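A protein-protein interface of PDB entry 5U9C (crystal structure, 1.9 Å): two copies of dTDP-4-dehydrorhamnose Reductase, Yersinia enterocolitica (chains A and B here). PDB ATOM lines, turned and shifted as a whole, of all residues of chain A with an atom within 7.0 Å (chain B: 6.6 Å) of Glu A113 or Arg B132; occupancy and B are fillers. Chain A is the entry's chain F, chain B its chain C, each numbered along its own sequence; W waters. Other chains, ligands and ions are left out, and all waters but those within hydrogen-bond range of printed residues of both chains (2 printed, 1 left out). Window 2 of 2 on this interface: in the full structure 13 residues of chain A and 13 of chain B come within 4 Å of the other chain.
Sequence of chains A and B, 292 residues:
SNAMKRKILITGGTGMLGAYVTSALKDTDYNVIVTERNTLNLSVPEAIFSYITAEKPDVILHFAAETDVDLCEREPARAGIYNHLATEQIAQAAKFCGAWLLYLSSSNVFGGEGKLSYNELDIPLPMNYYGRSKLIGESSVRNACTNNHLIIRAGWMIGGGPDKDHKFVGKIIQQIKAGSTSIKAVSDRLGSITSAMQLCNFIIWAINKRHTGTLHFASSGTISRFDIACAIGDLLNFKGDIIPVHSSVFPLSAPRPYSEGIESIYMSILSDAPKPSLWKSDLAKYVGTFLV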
ATOM      1  N   PHE A 110      10.846 -27.638  33.774  1.00  0.00           N
ATOM      2  CA  PHE A 110      10.593 -28.428  32.559  1.00  0.00           C
ATOM      3  C   PHE A 110       9.222 -29.119  32.646  1.00  0.00           C
ATOM      4  O   PHE A 110       8.626 -29.207  33.718  1.00  0.00           O
ATOM      5  CB  PHE A 110      11.651 -29.539  32.388  1.00  0.00           C
ATOM      6  CG  PHE A 110      13.056 -29.037  32.300  1.00  0.00           C
ATOM      7  CD1 PHE A 110      13.521 -28.456  31.134  1.00  0.00           C
ATOM      8  CD2 PHE A 110      13.930 -29.192  33.363  1.00  0.00           C
ATOM      9  CE1 PHE A 110      14.829 -27.998  31.039  1.00  0.00           C
ATOM     10  CE2 PHE A 110      15.241 -28.742  33.281  1.00  0.00           C
ATOM     11  CZ  PHE A 110      15.695 -28.153  32.110  1.00  0.00           C
ATOM     12  N   GLY A 111       8.757 -29.617  31.506  1.00  0.00           N
ATOM     13  CA  GLY A 111       7.525 -30.383  31.429  1.00  0.00           C
ATOM     14  C   GLY A 111       6.695 -30.089  30.203  1.00  0.00           C
ATOM     15  O   GLY A 111       6.027 -30.969  29.673  1.00  0.00           O
ATOM     16  N   GLY A 112       6.733 -28.835  29.765  1.00  0.00           N
ATOM     17  CA  GLY A 112       5.933 -28.405  28.639  1.00  0.00           C
ATOM     18  C   GLY A 112       6.198 -29.123  27.339  1.00  0.00           C
ATOM     19  O   GLY A 112       5.287 -29.333  26.576  1.00  0.00           O
ATOM     20  N   GLU A 113       7.446 -29.498  27.084  1.00  0.00           N
ATOM     21  CA  GLU A 113       7.769 -30.191  25.848  1.00  0.00           C
ATOM     22  C   GLU A 113       7.218 -31.616  25.830  1.00  0.00           C
ATOM     23  O   GLU A 113       6.946 -32.155  24.776  1.00  0.00           O
ATOM     24  CB  GLU A 113       9.278 -30.171  25.586  1.00  0.00           C
ATOM     25  CG  GLU A 113       9.666 -30.957  24.333  1.00  0.00           C
ATOM     26  CD  GLU A 113      11.159 -30.944  24.022  1.00  0.00           C
ATOM     27  OE1 GLU A 113      11.908 -30.161  24.658  1.00  0.00           O
ATOM     28  OE2 GLU A 113      11.568 -31.714  23.108  1.00  0.00           O
ATOM     29  N   GLY A 114       7.048 -32.233  26.997  1.00  0.00           N
ATOM     30  CA  GLY A 114       6.474 -33.571  27.038  1.00  0.00           C
ATOM     31  C   GLY A 114       7.425 -34.748  26.809  1.00  0.00           C
ATOM     32  O   GLY A 114       6.970 -35.862  26.632  1.00  0.00           O
ATOM     33  N   LYS A 115       8.733 -34.530  26.822  1.00  0.00           N
ATOM     34  CA  LYS A 115       9.630 -35.666  26.658  1.00  0.00           C
ATOM     35  C   LYS A 115       9.921 -36.323  28.016  1.00  0.00           C
ATOM     36  O   LYS A 115       9.491 -35.828  29.043  1.00  0.00           O
ATOM     37  CB  LYS A 115      10.886 -35.295  25.925  1.00  0.00           C
ATOM     38  CG  LYS A 115      11.810 -34.284  26.557  1.00  0.00           C
ATOM     39  CD  LYS A 115      13.022 -34.248  25.622  1.00  0.00           C
ATOM     40  CE  LYS A 115      14.059 -33.222  25.982  1.00  0.00           C
ATOM     41  NZ  LYS A 115      15.111 -33.293  24.930  1.00  0.00           N
ATOM     42  N   TYR A 118      15.168 -34.439  30.962  1.00  0.00           N
ATOM     43  CA  TYR A 118      15.783 -33.198  30.513  1.00  0.00           C
ATOM     44  C   TYR A 118      17.156 -33.022  31.140  1.00  0.00           C
ATOM     45  O   TYR A 118      17.329 -33.294  32.325  1.00  0.00           O
ATOM     46  CB  TYR A 118      14.892 -32.018  30.964  1.00  0.00           C
ATOM     47  CG  TYR A 118      13.496 -32.038  30.423  1.00  0.00           C
ATOM     48  CD1 TYR A 118      12.482 -32.722  31.073  1.00  0.00           C
ATOM     49  CD2 TYR A 118      13.182 -31.379  29.221  1.00  0.00           C
ATOM     50  CE1 TYR A 118      11.184 -32.739  30.562  1.00  0.00           C
ATOM     51  CE2 TYR A 118      11.896 -31.400  28.703  1.00  0.00           C
ATOM     52  CZ  TYR A 118      10.899 -32.080  29.365  1.00  0.00           C
ATOM     53  OH  TYR A 118       9.610 -32.086  28.825  1.00  0.00           O
ATOM     54  N   ASN A 119      18.121 -32.576  30.345  1.00  0.00           N
ATOM     55  CA  ASN A 119      19.461 -32.294  30.860  1.00  0.00           C
ATOM     56  C   ASN A 119      19.729 -30.763  30.809  1.00  0.00           C
ATOM     57  O   ASN A 119      18.868 -29.978  30.354  1.00  0.00           O
ATOM     58  CB  ASN A 119      20.527 -33.125  30.123  1.00  0.00           C
ATOM     59  CG  ASN A 119      20.662 -32.763  28.665  1.00  0.00           C
ATOM     60  OD1 ASN A 119      20.628 -31.585  28.300  1.00  0.00           O
ATOM     61  ND2 ASN A 119      20.854 -33.782  27.813  1.00  0.00           N
ATOM     62  N   LEU A 121      21.194 -28.835  28.890  1.00  0.00           N
ATOM     63  CA  LEU A 121      21.074 -28.165  27.589  1.00  0.00           C
ATOM     64  C   LEU A 121      19.624 -27.945  27.183  1.00  0.00           C
ATOM     65  O   LEU A 121      19.353 -27.158  26.273  1.00  0.00           O
ATOM     66  CB  LEU A 121      21.786 -28.948  26.468  1.00  0.00           C
ATOM     67  CG  LEU A 121      23.288 -28.842  26.435  1.00  0.00           C
ATOM     68  CD1 LEU A 121      23.847 -29.731  25.327  1.00  0.00           C
ATOM     69  CD2 LEU A 121      23.711 -27.377  26.236  1.00  0.00           C
ATOM     70  N   ASP A 122      18.693 -28.685  27.788  1.00  0.00           N
ATOM     71  CA  ASP A 122      17.288 -28.484  27.472  1.00  0.00           C
ATOM     72  C   ASP A 122      16.829 -27.082  27.936  1.00  0.00           C
ATOM     73  O   ASP A 122      17.250 -26.593  28.983  1.00  0.00           O
ATOM     74  CB  ASP A 122      16.441 -29.640  28.034  1.00  0.00           C
ATOM     75  CG  ASP A 122      16.622 -30.899  27.219  1.00  0.00           C
ATOM     76  OD1 ASP A 122      16.193 -30.885  26.052  1.00  0.00           O
ATOM     77  OD2 ASP A 122      17.241 -31.866  27.705  1.00  0.00           O
ATOM     78  N   ILE A 123      16.041 -26.421  27.102  1.00  0.00           N
ATOM     79  CA  ILE A 123      15.555 -25.074  27.400  1.00  0.00           C
ATOM     80  C   ILE A 123      14.309 -25.186  28.249  1.00  0.00           C
ATOM     81  O   ILE A 123      13.343 -25.749  27.815  1.00  0.00           O
ATOM     82  CB  ILE A 123      15.200 -24.308  26.115  1.00  0.00           C
ATOM     83  CG1 ILE A 123      16.354 -24.380  25.114  1.00  0.00           C
ATOM     84  CG2 ILE A 123      14.805 -22.851  26.423  1.00  0.00           C
ATOM     85  CD1 ILE A 123      17.684 -23.919  25.652  1.00  0.00           C
ATOM     86  N   LEU A 125      10.736 -24.963  29.850  1.00  0.00           N
ATOM     87  CA  LEU A 125       9.393 -24.632  29.361  1.00  0.00           C
ATOM     88  C   LEU A 125       8.451 -25.212  30.421  1.00  0.00           C
ATOM     89  O   LEU A 125       8.051 -26.378  30.330  1.00  0.00           O
ATOM     90  CB  LEU A 125       9.132 -25.260  27.992  1.00  0.00           C
ATOM     91  CG  LEU A 125       7.773 -25.021  27.334  1.00  0.00           C
ATOM     92  CD1 LEU A 125       7.465 -23.532  27.243  1.00  0.00           C
ATOM     93  CD2 LEU A 125       7.732 -25.655  25.944  1.00  0.00           C
ATOM     94  N   PRO A 126       8.131 -24.427  31.459  1.00  0.00           N
ATOM     95  CA  PRO A 126       7.292 -24.952  32.546  1.00  0.00           C
ATOM     96  C   PRO A 126       5.835 -25.269  32.173  1.00  0.00           C
ATOM     97  O   PRO A 126       5.346 -24.858  31.120  1.00  0.00           O
ATOM     98  CB  PRO A 126       7.348 -23.846  33.601  1.00  0.00           C
ATOM     99  CG  PRO A 126       8.549 -23.045  33.263  1.00  0.00           C
ATOM    100  CD  PRO A 126       8.652 -23.090  31.775  1.00  0.00           C
ATOM    101  N   MET A 127       5.181 -26.006  33.060  1.00  0.00           N
ATOM    102  CA  MET A 127       3.786 -26.457  32.891  1.00  0.00           C
ATOM    103  C   MET A 127       2.828 -25.843  33.893  1.00  0.00           C
ATOM    104  O   MET A 127       1.624 -26.000  33.759  1.00  0.00           O
ATOM    105  CB  MET A 127       3.858 -27.970  33.132  1.00  0.00           C
ATOM    106  CG  MET A 127       2.654 -28.767  32.655  1.00  0.00           C
ATOM    107  SD  MET A 127       3.023 -29.677  30.951  1.00  0.00           S
ATOM    108  CE  MET A 127       1.135 -30.174  30.736  1.00  0.00           C
ATOM    109  N   PRO A 257       3.332 -32.389  34.382  1.00  0.00           N
ATOM    110  CA  PRO A 257       3.693 -32.889  33.051  1.00  0.00           C
ATOM    111  C   PRO A 257       3.777 -34.421  33.030  1.00  0.00           C
ATOM    112  O   PRO A 257       3.869 -35.046  34.092  1.00  0.00           O
ATOM    113  CB  PRO A 257       5.083 -32.317  32.845  1.00  0.00           C
ATOM    114  CG  PRO A 257       5.682 -32.289  34.215  1.00  0.00           C
ATOM    115  CD  PRO A 257       4.527 -32.014  35.162  1.00  0.00           C
ATOM    116  N   GLU B  73      23.984 -35.041  19.443  1.00  0.00           N
ATOM    117  CA  GLU B  73      22.768 -35.677  19.909  1.00  0.00           C
ATOM    118  C   GLU B  73      23.066 -36.927  20.731  1.00  0.00           C
ATOM    119  O   GLU B  73      22.410 -37.173  21.730  1.00  0.00           O
ATOM    120  CB  GLU B  73      21.853 -36.052  18.737  1.00  0.00           C
ATOM    121  CG  GLU B  73      20.410 -36.287  19.178  1.00  0.00           C
ATOM    122  CD  GLU B  73      19.676 -34.991  19.519  1.00  0.00           C
ATOM    123  OE1 GLU B  73      20.220 -33.865  19.304  1.00  0.00           O
ATOM    124  OE2 GLU B  73      18.545 -35.106  20.003  1.00  0.00           O
ATOM    125  N   HIS B  84      28.795 -24.747  24.976  1.00  0.00           N
ATOM    126  CA  HIS B  84      28.219 -23.939  26.049  1.00  0.00           C
ATOM    127  C   HIS B  84      29.247 -23.528  27.097  1.00  0.00           C
ATOM    128  O   HIS B  84      29.563 -22.338  27.207  1.00  0.00           O
ATOM    129  CB  HIS B  84      26.999 -24.659  26.650  1.00  0.00           C
ATOM    130  CG  HIS B  84      26.512 -24.089  27.939  1.00  0.00           C
ATOM    131  ND1 HIS B  84      25.890 -24.867  28.890  1.00  0.00           N
ATOM    132  CD2 HIS B  84      26.586 -22.838  28.457  1.00  0.00           C
ATOM    133  CE1 HIS B  84      25.569 -24.110  29.927  1.00  0.00           C
ATOM    134  NE2 HIS B  84      25.984 -22.878  29.694  1.00  0.00           N
ATOM    135  N   ASN B 108      20.610 -23.418  13.186  1.00  0.00           N
ATOM    136  CA  ASN B 108      20.073 -24.531  14.014  1.00  0.00           C
ATOM    137  C   ASN B 108      19.544 -24.118  15.383  1.00  0.00           C
ATOM    138  O   ASN B 108      19.080 -24.966  16.147  1.00  0.00           O
ATOM    139  CB  ASN B 108      21.103 -25.671  14.179  1.00  0.00           C
ATOM    140  CG  ASN B 108      20.854 -26.839  13.257  1.00  0.00           C
ATOM    141  OD1 ASN B 108      19.874 -27.586  13.445  1.00  0.00           O
ATOM    142  ND2 ASN B 108      21.789 -27.099  12.346  1.00  0.00           N
ATOM    143  N   VAL B 109      19.647 -22.847  15.736  1.00  0.00           N
ATOM    144  CA  VAL B 109      18.988 -22.389  16.974  1.00  0.00           C
ATOM    145  C   VAL B 109      17.467 -22.322  16.709  1.00  0.00           C
ATOM    146  O   VAL B 109      16.699 -22.160  17.638  1.00  0.00           O
ATOM    147  CB  VAL B 109      19.469 -21.021  17.513  1.00  0.00           C
ATOM    148  CG1 VAL B 109      20.936 -21.072  17.914  1.00  0.00           C
ATOM    149  CG2 VAL B 109      19.190 -19.903  16.513  1.00  0.00           C
ATOM    150  N   PRO B 126      15.186 -24.351  19.455  1.00  0.00           N
ATOM    151  CA  PRO B 126      15.905 -25.411  18.740  1.00  0.00           C
ATOM    152  C   PRO B 126      15.181 -26.763  18.635  1.00  0.00           C
ATOM    153  O   PRO B 126      14.177 -26.992  19.312  1.00  0.00           O
ATOM    154  CB  PRO B 126      17.221 -25.528  19.520  1.00  0.00           C
ATOM    155  CG  PRO B 126      16.926 -24.980  20.873  1.00  0.00           C
ATOM    156  CD  PRO B 126      15.886 -23.924  20.677  1.00  0.00           C
ATOM    157  N   MET B 127      15.718 -27.620  17.764  1.00  0.00           N
ATOM    158  CA  MET B 127      15.199 -28.973  17.475  1.00  0.00           C
ATOM    159  C   MET B 127      16.102 -30.091  17.952  1.00  0.00           C
ATOM    160  O   MET B 127      15.679 -31.243  17.987  1.00  0.00           O
ATOM    161  CB  MET B 127      15.140 -29.075  15.940  1.00  0.00           C
ATOM    162  CG  MET B 127      14.386 -30.279  15.350  1.00  0.00           C
ATOM    163  SD  MET B 127      12.527 -29.762  14.963  1.00  0.00           S
ATOM    164  CE  MET B 127      11.896 -31.467  14.212  1.00  0.00           C
ATOM    165  N   ASN B 128      17.352 -29.772  18.284  1.00  0.00           N
ATOM    166  CA  ASN B 128      18.333 -30.785  18.705  1.00  0.00           C
ATOM    167  C   ASN B 128      19.392 -30.223  19.653  1.00  0.00           C
ATOM    168  O   ASN B 128      19.482 -29.005  19.837  1.00  0.00           O
ATOM    169  CB  ASN B 128      18.977 -31.444  17.471  1.00  0.00           C
ATOM    170  CG  ASN B 128      19.640 -30.451  16.533  1.00  0.00           C
ATOM    171  OD1 ASN B 128      20.370 -29.541  16.953  1.00  0.00           O
ATOM    172  ND2 ASN B 128      19.439 -30.659  15.235  1.00  0.00           N
ATOM    173  N   TYR B 129      20.183 -31.111  20.255  1.00  0.00           N
ATOM    174  CA  TYR B 129      21.229 -30.696  21.208  1.00  0.00           C
ATOM    175  C   TYR B 129      22.286 -29.783  20.645  1.00  0.00           C
ATOM    176  O   TYR B 129      22.765 -28.888  21.350  1.00  0.00           O
ATOM    177  CB  TYR B 129      21.826 -31.895  21.990  1.00  0.00           C
ATOM    178  CG  TYR B 129      20.861 -32.387  23.036  1.00  0.00           C
ATOM    179  CD1 TYR B 129      20.522 -31.583  24.105  1.00  0.00           C
ATOM    180  CD2 TYR B 129      20.250 -33.645  22.938  1.00  0.00           C
ATOM    181  CE1 TYR B 129      19.595 -32.002  25.069  1.00  0.00           C
ATOM    182  CE2 TYR B 129      19.331 -34.086  23.902  1.00  0.00           C
ATOM    183  CZ  TYR B 129      19.008 -33.258  24.967  1.00  0.00           C
ATOM    184  OH  TYR B 129      18.082 -33.672  25.919  1.00  0.00           O
ATOM    185  N   TYR B 130      22.672 -29.991  19.385  1.00  0.00           N
ATOM    186  CA  TYR B 130      23.610 -29.060  18.785  1.00  0.00           C
ATOM    187  C   TYR B 130      23.029 -27.644  18.846  1.00  0.00           C
ATOM    188  O   TYR B 130      23.677 -26.714  19.352  1.00  0.00           O
ATOM    189  CB  TYR B 130      23.877 -29.401  17.340  1.00  0.00           C
ATOM    190  CG  TYR B 130      24.641 -28.321  16.637  1.00  0.00           C
ATOM    191  CD1 TYR B 130      25.946 -28.021  17.007  1.00  0.00           C
ATOM    192  CD2 TYR B 130      24.075 -27.615  15.567  1.00  0.00           C
ATOM    193  CE1 TYR B 130      26.672 -27.040  16.342  1.00  0.00           C
ATOM    194  CE2 TYR B 130      24.795 -26.621  14.898  1.00  0.00           C
ATOM    195  CZ  TYR B 130      26.082 -26.331  15.290  1.00  0.00           C
ATOM    196  OH  TYR B 130      26.794 -25.347  14.635  1.00  0.00           O
ATOM    197  N   GLY B 131      21.800 -27.492  18.342  1.00  0.00           N
ATOM    198  CA  GLY B 131      21.109 -26.198  18.324  1.00  0.00           C
ATOM    199  C   GLY B 131      20.985 -25.582  19.714  1.00  0.00           C
ATOM    200  O   GLY B 131      21.220 -24.391  19.897  1.00  0.00           O
ATOM    201  N   ARG B 132      20.625 -26.405  20.699  1.00  0.00           N
ATOM    202  CA  ARG B 132      20.509 -25.932  22.080  1.00  0.00           C
ATOM    203  C   ARG B 132      21.857 -25.461  22.626  1.00  0.00           C
ATOM    204  O   ARG B 132      21.915 -24.478  23.370  1.00  0.00           O
ATOM    205  CB  ARG B 132      19.967 -27.028  22.989  1.00  0.00           C
ATOM    206  CG  ARG B 132      18.504 -27.410  22.728  1.00  0.00           C
ATOM    207  CD  ARG B 132      18.086 -28.657  23.498  1.00  0.00           C
ATOM    208  NE  ARG B 132      16.773 -29.099  23.058  1.00  0.00           N
ATOM    209  CZ  ARG B 132      16.452 -30.289  22.565  1.00  0.00           C
ATOM    210  NH1 ARG B 132      17.310 -31.304  22.533  1.00  0.00           N
ATOM    211  NH2 ARG B 132      15.195 -30.505  22.193  1.00  0.00           N
ATOM    212  N   SER B 133      22.932 -26.183  22.290  1.00  0.00           N
ATOM    213  CA  SER B 133      24.260 -25.826  22.781  1.00  0.00           C
ATOM    214  C   SER B 133      24.733 -24.489  22.188  1.00  0.00           C
ATOM    215  O   SER B 133      25.341 -23.678  22.881  1.00  0.00           O
ATOM    216  CB  SER B 133      25.290 -26.952  22.554  1.00  0.00           C
ATOM    217  OG  SER B 133      25.659 -27.067  21.200  1.00  0.00           O
ATOM    218  N   LYS B 134      24.426 -24.252  20.919  1.00  0.00           N
ATOM    219  CA  LYS B 134      24.768 -22.990  20.285  1.00  0.00           C
ATOM    220  C   LYS B 134      23.943 -21.831  20.889  1.00  0.00           C
ATOM    221  O   LYS B 134      24.487 -20.761  21.159  1.00  0.00           O
ATOM    222  CB  LYS B 134      24.562 -23.071  18.785  1.00  0.00           C
ATOM    223  CG  LYS B 134      25.507 -24.025  18.085  1.00  0.00           C
ATOM    224  CD  LYS B 134      26.993 -23.706  18.262  1.00  0.00           C
ATOM    225  CE  LYS B 134      27.336 -22.368  17.653  1.00  0.00           C
ATOM    226  NZ  LYS B 134      28.800 -22.199  17.517  1.00  0.00           N
ATOM    227  N   LEU B 135      22.656 -22.078  21.136  1.00  0.00           N
ATOM    228  CA  LEU B 135      21.769 -21.067  21.693  1.00  0.00           C
ATOM    229  C   LEU B 135      22.194 -20.662  23.093  1.00  0.00           C
ATOM    230  O   LEU B 135      22.250 -19.475  23.392  1.00  0.00           O
ATOM    231  CB  LEU B 135      20.322 -21.559  21.738  1.00  0.00           C
ATOM    232  CG  LEU B 135      19.286 -20.550  22.282  1.00  0.00           C
ATOM    233  CD1 LEU B 135      19.310 -19.242  21.484  1.00  0.00           C
ATOM    234  CD2 LEU B 135      17.904 -21.160  22.246  1.00  0.00           C
ATOM    235  N   ILE B 136      22.481 -21.641  23.950  1.00  0.00           N
ATOM    236  CA  ILE B 136      22.899 -21.333  25.308  1.00  0.00           C
ATOM    237  C   ILE B 136      24.261 -20.600  25.238  1.00  0.00           C
ATOM    238  O   ILE B 136      24.519 -19.684  26.033  1.00  0.00           O
ATOM    239  CB  ILE B 136      22.870 -22.565  26.233  1.00  0.00           C
ATOM    240  CG1 ILE B 136      21.425 -23.063  26.356  1.00  0.00           C
ATOM    241  CG2 ILE B 136      23.328 -22.177  27.630  1.00  0.00           C
ATOM    242  CD1 ILE B 136      21.258 -24.402  27.048  1.00  0.00           C
ATOM    243  N   GLY B 137      25.098 -20.974  24.261  1.00  0.00           N
ATOM    244  CA  GLY B 137      26.343 -20.234  23.999  1.00  0.00           C
ATOM    245  C   GLY B 137      26.052 -18.763  23.701  1.00  0.00           C
ATOM    246  O   GLY B 137      26.705 -17.885  24.265  1.00  0.00           O
HETATM  247  O   HOH W   1      12.764 -28.640  22.130  1.00  0.00           O
HETATM  248  O   HOH W   2      13.905 -32.902  22.440  1.00  0.00           O
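Glu A113 touches just one residue of chain B: Arg B132. Printed residues of chain B within 4 Å of Asp A122: Tyr B129 and Arg B132. Of the printed residues of chain B, Ile A123 touches Ile B136. Glu B73 touches none of the printed residues of chain A. No residue of chain A comes within 4 Å of Gly B131. Arg B132 touches just these residues of chain A: Glu A113 (3.9 Å), Lys A115 (3.8 Å), Leu A121 (3.3 Å) and Asp A122 (3.5 Å). Leu B135 touches none of the printed residues of chain A. The nearest printed residue of chain B that does not touch Glu A113 is Met B127 (6.6 Å).
N of Lys A115 lies within hydrogen-bond range of OH of Tyr A118. O of Tyr B129 lies close to OG of Ser B133. NZ of Lys A115 lies within salt-bridge range of OD1 of Asp A122 (2.9 Å). O of Tyr B130 is in hydrogen-bond range of OG of Ser B133, at 2.7 Å. The side-chain amide oxygen (OD1) of Asn A119 sits at hydrogen-bond distance from the backbone NH (N) of Leu A121, at 2.9 Å. N of Asn A119 sits at hydrogen-bond distance from OD2 of Asp A122, 2.9 Å away.
Hydrophobic or aromatic side chains of chain A within 4 Å of the printed part of chain B: Leu A121 and Ile A123. Of the 16 printed residues of chain B, 4 touch a printed residue of chain A. Among the printed residues, 11 pairs touch across the chains.
The side-chain amide nitrogen (ND2) of Asn A119 sits at hydrogen-bond distance from the side-chain hydroxyl (OH) of Tyr B129 (3.4 Å). OD1 of Asp A122 is in salt-bridge range of NE of Arg B132 (3.5 Å). The side-chain carboxylate of Glu A113 lies within salt-bridge range of the guanidinium group of Arg B132 (3.9 Å). The side-chain hydroxyl of Tyr B129 is in hydrogen-bond range of the side-chain carboxylate of Asp A122 (2.7 Å). NZ of Lys A115 is in hydrogen-bond range of OH of Tyr B129, at 3.2 Å.
Positions printed for both chains: 126 and 127. Of the 11 pairs that touch across the chains among the printed residues, none has its exchanged pair printed and touching as well.
Among the printed residues, pairs that only touch across the chains: Lys A115 with Arg B132, Leu A121 with Tyr B129, Leu A121 with Arg B132, Leu A121 with Ser B133, Leu A121 with Ile B136 and Ile A123 with Ile B136.
Water W2 lies within hydrogen-bond range of OE2 of Glu A113 (2.7 Å), NH2 of Arg B132 (2.7 Å) and NZ of Lys A115 (2.8 Å). Water W1 bridges the guanidinium group (NH2) of Arg B132 and the side-chain carboxylate (OE1) of Glu A113.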
